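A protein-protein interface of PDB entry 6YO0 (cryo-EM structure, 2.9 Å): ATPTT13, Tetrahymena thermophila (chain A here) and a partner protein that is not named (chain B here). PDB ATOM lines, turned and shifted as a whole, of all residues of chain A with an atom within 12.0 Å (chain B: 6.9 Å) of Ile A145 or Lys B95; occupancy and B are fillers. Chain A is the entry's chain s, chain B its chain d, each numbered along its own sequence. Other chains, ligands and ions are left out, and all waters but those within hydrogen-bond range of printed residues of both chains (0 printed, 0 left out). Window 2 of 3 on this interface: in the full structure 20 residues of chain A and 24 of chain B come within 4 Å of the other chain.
The backbone carbonyl oxygen (O) of Leu A144 lies within hydrogen-bond range of the side-chain amide nitrogen (ND2) of Asn B99, 3.2 Å away.
The backbone carbonyl oxygen (O) of Asp A143 lies close to the side-chain amide nitrogen (ND2) of Asn B99 (2.3 Å).
O of Val B96 touches CD1 of Leu A144 (3.9 Å).
Leu A144 touches Tyr B100.
Lys B95 touches Ile A145.
Ile A145 touches Val B96.
Of the 8 printed residues of chain A, 3 touch a printed residue of chain B.
Hydrophobic or aromatic side chains of chain A that line the printed part of chain B: Leu A144 and Ile A145.
Printed residues of chain B that touch a printed residue of chain A: Lys B95, Val B96, Asn B99 and Tyr B100.
Hydrophobic or aromatic side chains of chain B within 4 Å of the printed part of chain A: Val B96 and Tyr B100.
Of the printed residues of chain B, Asp A143 touches Asn B99 (2.3 Å).
Printed residues of chain B within 4 Å of Leu A144: Val B96 (3.9 Å), Asn B99 (3.2 Å) and Tyr B100 (3.6 Å).
Printed residues of chain B within 4 Å of Ile A145: Lys B95 and Val B96.
No residue of chain A comes within 4 Å of Leu B92.
No residue of chain A comes within 4 Å of Val B93.
No residue of chain A comes within 4 Å of Asp B94.
Lys B95 touches just one residue of chain A: Ile A145 (3.6 Å).
Glu B98 touches none of the printed residues of chain A.
Of chain A, only Asp A143 (2.3 Å) and Leu A144 (3.2 Å) come within 4 Å of Asn B99.
Printed residues of chain A within 4 Å of Tyr B100: Leu A144.
The nearest residue of chain A that does not touch Lys B95 is Leu A144 (4.8 Å).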
ATOM      1  N   ILE A 138      21.701 -19.912 -28.789  1.00  0.00           N
ATOM      2  CA  ILE A 138      20.809 -20.946 -28.273  1.00  0.00           C
ATOM      3  C   ILE A 138      21.465 -21.699 -27.126  1.00  0.00           C
ATOM      4  O   ILE A 138      20.807 -22.061 -26.144  1.00  0.00           O
ATOM      5  CB  ILE A 138      20.380 -21.899 -29.402  1.00  0.00           C
ATOM      6  CG1 ILE A 138      19.702 -21.113 -30.526  1.00  0.00           C
ATOM      7  CG2 ILE A 138      19.468 -22.976 -28.844  1.00  0.00           C
ATOM      8  CD1 ILE A 138      19.335 -21.946 -31.740  1.00  0.00           C
ATOM      9  N   LEU A 139      22.767 -21.956 -27.231  1.00  0.00           N
ATOM     10  CA  LEU A 139      23.442 -22.741 -26.206  1.00  0.00           C
ATOM     11  C   LEU A 139      23.857 -21.872 -25.029  1.00  0.00           C
ATOM     12  O   LEU A 139      23.901 -22.354 -23.892  1.00  0.00           O
ATOM     13  CB  LEU A 139      24.647 -23.465 -26.807  1.00  0.00           C
ATOM     14  CG  LEU A 139      24.321 -24.404 -27.975  1.00  0.00           C
ATOM     15  CD1 LEU A 139      25.539 -25.201 -28.398  1.00  0.00           C
ATOM     16  CD2 LEU A 139      23.185 -25.341 -27.609  1.00  0.00           C
ATOM     17  N   SER A 140      24.157 -20.598 -25.279  1.00  0.00           N
ATOM     18  CA  SER A 140      24.358 -19.646 -24.196  1.00  0.00           C
ATOM     19  C   SER A 140      23.054 -19.295 -23.496  1.00  0.00           C
ATOM     20  O   SER A 140      23.089 -18.691 -22.419  1.00  0.00           O
ATOM     21  CB  SER A 140      25.018 -18.376 -24.730  1.00  0.00           C
ATOM     22  OG  SER A 140      26.257 -18.672 -25.349  1.00  0.00           O
ATOM     23  N   LYS A 141      21.912 -19.655 -24.086  1.00  0.00           N
ATOM     24  CA  LYS A 141      20.620 -19.426 -23.449  1.00  0.00           C
ATOM     25  C   LYS A 141      20.583 -20.044 -22.059  1.00  0.00           C
ATOM     26  O   LYS A 141      20.399 -19.353 -21.052  1.00  0.00           O
ATOM     27  CB  LYS A 141      19.509 -20.019 -24.319  1.00  0.00           C
ATOM     28  CG  LYS A 141      18.116 -19.960 -23.708  1.00  0.00           C
ATOM     29  CD  LYS A 141      17.682 -18.546 -23.365  1.00  0.00           C
ATOM     30  CE  LYS A 141      17.822 -17.608 -24.551  1.00  0.00           C
ATOM     31  NZ  LYS A 141      17.092 -18.122 -25.742  1.00  0.00           N
ATOM     32  N   GLY A 142      20.760 -21.361 -21.996  1.00  0.00           N
ATOM     33  CA  GLY A 142      20.691 -22.080 -20.744  1.00  0.00           C
ATOM     34  C   GLY A 142      21.797 -23.110 -20.670  1.00  0.00           C
ATOM     35  O   GLY A 142      22.341 -23.548 -21.687  1.00  0.00           O
ATOM     36  N   ASP A 143      22.123 -23.493 -19.442  1.00  0.00           N
ATOM     37  CA  ASP A 143      23.119 -24.523 -19.187  1.00  0.00           C
ATOM     38  C   ASP A 143      22.369 -25.785 -18.783  1.00  0.00           C
ATOM     39  O   ASP A 143      21.614 -25.784 -17.805  1.00  0.00           O
ATOM     40  CB  ASP A 143      24.101 -24.092 -18.100  1.00  0.00           C
ATOM     41  CG  ASP A 143      25.177 -25.125 -17.845  1.00  0.00           C
ATOM     42  OD1 ASP A 143      25.168 -26.176 -18.520  1.00  0.00           O
ATOM     43  OD2 ASP A 143      26.035 -24.888 -16.969  1.00  0.00           O
ATOM     44  N   LEU A 144      22.586 -26.855 -19.547  1.00  0.00           N
ATOM     45  CA  LEU A 144      21.840 -28.092 -19.356  1.00  0.00           C
ATOM     46  C   LEU A 144      21.948 -28.601 -17.923  1.00  0.00           C
ATOM     47  O   LEU A 144      20.944 -28.680 -17.205  1.00  0.00           O
ATOM     48  CB  LEU A 144      22.347 -29.139 -20.345  1.00  0.00           C
ATOM     49  CG  LEU A 144      21.619 -30.476 -20.349  1.00  0.00           C
ATOM     50  CD1 LEU A 144      20.131 -30.262 -20.580  1.00  0.00           C
ATOM     51  CD2 LEU A 144      22.215 -31.364 -21.416  1.00  0.00           C
ATOM     52  N   ILE A 145      23.158 -28.949 -17.494  1.00  0.00           N
ATOM     53  CA  ILE A 145      23.412 -29.499 -16.158  1.00  0.00           C
ATOM     54  C   ILE A 145      22.292 -30.437 -15.729  1.00  0.00           C
ATOM     55  O   ILE A 145      21.660 -31.079 -16.565  1.00  0.00           O
ATOM     56  CB  ILE A 145      23.627 -28.384 -15.098  1.00  0.00           C
ATOM     57  CG1 ILE A 145      22.417 -27.449 -14.971  1.00  0.00           C
ATOM     58  CG2 ILE A 145      24.858 -27.582 -15.444  1.00  0.00           C
ATOM     59  CD1 ILE A 145      21.297 -27.989 -14.105  1.00  0.00           C
ATOM     60  N   GLY B  91      15.113 -34.898  -8.094  1.00  0.00           N
ATOM     61  CA  GLY B  91      15.126 -33.592  -8.713  1.00  0.00           C
ATOM     62  C   GLY B  91      16.113 -33.427  -9.846  1.00  0.00           C
ATOM     63  O   GLY B  91      16.019 -32.443 -10.591  1.00  0.00           O
ATOM     64  N   LEU B  92      17.054 -34.355 -10.004  1.00  0.00           N
ATOM     65  CA  LEU B  92      18.056 -34.225 -11.052  1.00  0.00           C
ATOM     66  C   LEU B  92      17.461 -34.544 -12.415  1.00  0.00           C
ATOM     67  O   LEU B  92      17.642 -33.786 -13.375  1.00  0.00           O
ATOM     68  CB  LEU B  92      19.241 -35.141 -10.746  1.00  0.00           C
ATOM     69  CG  LEU B  92      20.450 -35.079 -11.679  1.00  0.00           C
ATOM     70  CD1 LEU B  92      21.670 -35.635 -10.975  1.00  0.00           C
ATOM     71  CD2 LEU B  92      20.197 -35.839 -12.966  1.00  0.00           C
ATOM     72  N   VAL B  93      16.740 -35.661 -12.517  1.00  0.00           N
ATOM     73  CA  VAL B  93      16.184 -36.072 -13.801  1.00  0.00           C
ATOM     74  C   VAL B  93      15.201 -35.025 -14.305  1.00  0.00           C
ATOM     75  O   VAL B  93      15.214 -34.654 -15.484  1.00  0.00           O
ATOM     76  CB  VAL B  93      15.525 -37.460 -13.682  1.00  0.00           C
ATOM     77  CG1 VAL B  93      14.405 -37.443 -12.649  1.00  0.00           C
ATOM     78  CG2 VAL B  93      15.008 -37.919 -15.033  1.00  0.00           C
ATOM     79  N   ASP B  94      14.336 -34.530 -13.418  1.00  0.00           N
ATOM     80  CA  ASP B  94      13.343 -33.543 -13.827  1.00  0.00           C
ATOM     81  C   ASP B  94      14.007 -32.229 -14.212  1.00  0.00           C
ATOM     82  O   ASP B  94      13.590 -31.573 -15.174  1.00  0.00           O
ATOM     83  CB  ASP B  94      12.329 -33.328 -12.706  1.00  0.00           C
ATOM     84  CG  ASP B  94      11.577 -34.595 -12.350  1.00  0.00           C
ATOM     85  OD1 ASP B  94      12.152 -35.452 -11.644  1.00  0.00           O
ATOM     86  OD2 ASP B  94      10.412 -34.739 -12.779  1.00  0.00           O
ATOM     87  N   LYS B  95      15.044 -31.830 -13.475  1.00  0.00           N
ATOM     88  CA  LYS B  95      15.756 -30.603 -13.812  1.00  0.00           C
ATOM     89  C   LYS B  95      16.433 -30.726 -15.168  1.00  0.00           C
ATOM     90  O   LYS B  95      16.404 -29.792 -15.977  1.00  0.00           O
ATOM     91  CB  LYS B  95      16.780 -30.286 -12.726  1.00  0.00           C
ATOM     92  CG  LYS B  95      17.699 -29.124 -13.054  1.00  0.00           C
ATOM     93  CD  LYS B  95      18.562 -28.728 -11.864  1.00  0.00           C
ATOM     94  CE  LYS B  95      19.348 -29.901 -11.297  1.00  0.00           C
ATOM     95  NZ  LYS B  95      20.147 -29.506 -10.108  1.00  0.00           N
ATOM     96  N   VAL B  96      17.070 -31.867 -15.425  1.00  0.00           N
ATOM     97  CA  VAL B  96      17.677 -32.100 -16.730  1.00  0.00           C
ATOM     98  C   VAL B  96      16.615 -32.060 -17.819  1.00  0.00           C
ATOM     99  O   VAL B  96      16.821 -31.480 -18.893  1.00  0.00           O
ATOM    100  CB  VAL B  96      18.427 -33.444 -16.732  1.00  0.00           C
ATOM    101  CG1 VAL B  96      18.859 -33.803 -18.135  1.00  0.00           C
ATOM    102  CG2 VAL B  96      19.623 -33.387 -15.807  1.00  0.00           C
ATOM    103  N   LYS B  97      15.460 -32.670 -17.554  1.00  0.00           N
ATOM    104  CA  LYS B  97      14.387 -32.717 -18.542  1.00  0.00           C
ATOM    105  C   LYS B  97      13.872 -31.322 -18.876  1.00  0.00           C
ATOM    106  O   LYS B  97      13.726 -30.969 -20.052  1.00  0.00           O
ATOM    107  CB  LYS B  97      13.257 -33.599 -18.016  1.00  0.00           C
ATOM    108  CG  LYS B  97      12.029 -33.661 -18.898  1.00  0.00           C
ATOM    109  CD  LYS B  97      10.973 -34.555 -18.275  1.00  0.00           C
ATOM    110  CE  LYS B  97       9.730 -34.639 -19.135  1.00  0.00           C
ATOM    111  NZ  LYS B  97      10.040 -35.134 -20.502  1.00  0.00           N
ATOM    112  N   GLU B  98      13.590 -30.511 -17.856  1.00  0.00           N
ATOM    113  CA  GLU B  98      13.060 -29.176 -18.119  1.00  0.00           C
ATOM    114  C   GLU B  98      14.083 -28.305 -18.835  1.00  0.00           C
ATOM    115  O   GLU B  98      13.730 -27.548 -19.747  1.00  0.00           O
ATOM    116  CB  GLU B  98      12.606 -28.514 -16.818  1.00  0.00           C
ATOM    117  CG  GLU B  98      13.663 -28.438 -15.725  1.00  0.00           C
ATOM    118  CD  GLU B  98      14.592 -27.247 -15.872  1.00  0.00           C
ATOM    119  OE1 GLU B  98      14.296 -26.350 -16.689  1.00  0.00           O
ATOM    120  OE2 GLU B  98      15.625 -27.207 -15.169  1.00  0.00           O
ATOM    121  N   ASN B  99      15.355 -28.394 -18.443  1.00  0.00           N
ATOM    122  CA  ASN B  99      16.374 -27.592 -19.111  1.00  0.00           C
ATOM    123  C   ASN B  99      16.603 -28.080 -20.533  1.00  0.00           C
ATOM    124  O   ASN B  99      16.724 -27.273 -21.462  1.00  0.00           O
ATOM    125  CB  ASN B  99      17.676 -27.636 -18.315  1.00  0.00           C
ATOM    126  CG  ASN B  99      18.650 -26.555 -18.732  1.00  0.00           C
ATOM    127  OD1 ASN B  99      18.781 -26.245 -19.916  1.00  0.00           O
ATOM    128  ND2 ASN B  99      19.341 -25.974 -17.760  1.00  0.00           N
ATOM    129  N   TYR B 100      16.665 -29.397 -20.721  1.00  0.00           N
ATOM    130  CA  TYR B 100      16.772 -29.948 -22.066  1.00  0.00           C
ATOM    131  C   TYR B 100      15.591 -29.526 -22.927  1.00  0.00           C
ATOM    132  O   TYR B 100      15.765 -29.123 -24.082  1.00  0.00           O
ATOM    133  CB  TYR B 100      16.859 -31.470 -21.988  1.00  0.00           C
ATOM    134  CG  TYR B 100      16.489 -32.190 -23.260  1.00  0.00           C
ATOM    135  CD1 TYR B 100      17.423 -32.395 -24.262  1.00  0.00           C
ATOM    136  CD2 TYR B 100      15.208 -32.683 -23.450  1.00  0.00           C
ATOM    137  CE1 TYR B 100      17.090 -33.063 -25.421  1.00  0.00           C
ATOM    138  CE2 TYR B 100      14.865 -33.351 -24.604  1.00  0.00           C
ATOM    139  CZ  TYR B 100      15.809 -33.538 -25.587  1.00  0.00           C
ATOM    140  OH  TYR B 100      15.467 -34.204 -26.741  1.00  0.00           O
ATOM    141  N   GLU B 101      14.381 -29.580 -22.368  1.00  0.00           N
ATOM    142  CA  GLU B 101      13.194 -29.195 -23.124  1.00  0.00           C
ATOM    143  C   GLU B 101      13.230 -27.721 -23.505  1.00  0.00           C
ATOM    144  O   GLU B 101      12.882 -27.354 -24.633  1.00  0.00           O
ATOM    145  CB  GLU B 101      11.938 -29.507 -22.309  1.00  0.00           C
ATOM    146  CG  GLU B 101      10.629 -29.186 -23.015  1.00  0.00           C
ATOM    147  CD  GLU B 101      10.408 -30.015 -24.266  1.00  0.00           C
ATOM    148  OE1 GLU B 101      11.283 -30.838 -24.608  1.00  0.00           O
ATOM    149  OE2 GLU B 101       9.354 -29.841 -24.913  1.00  0.00           O
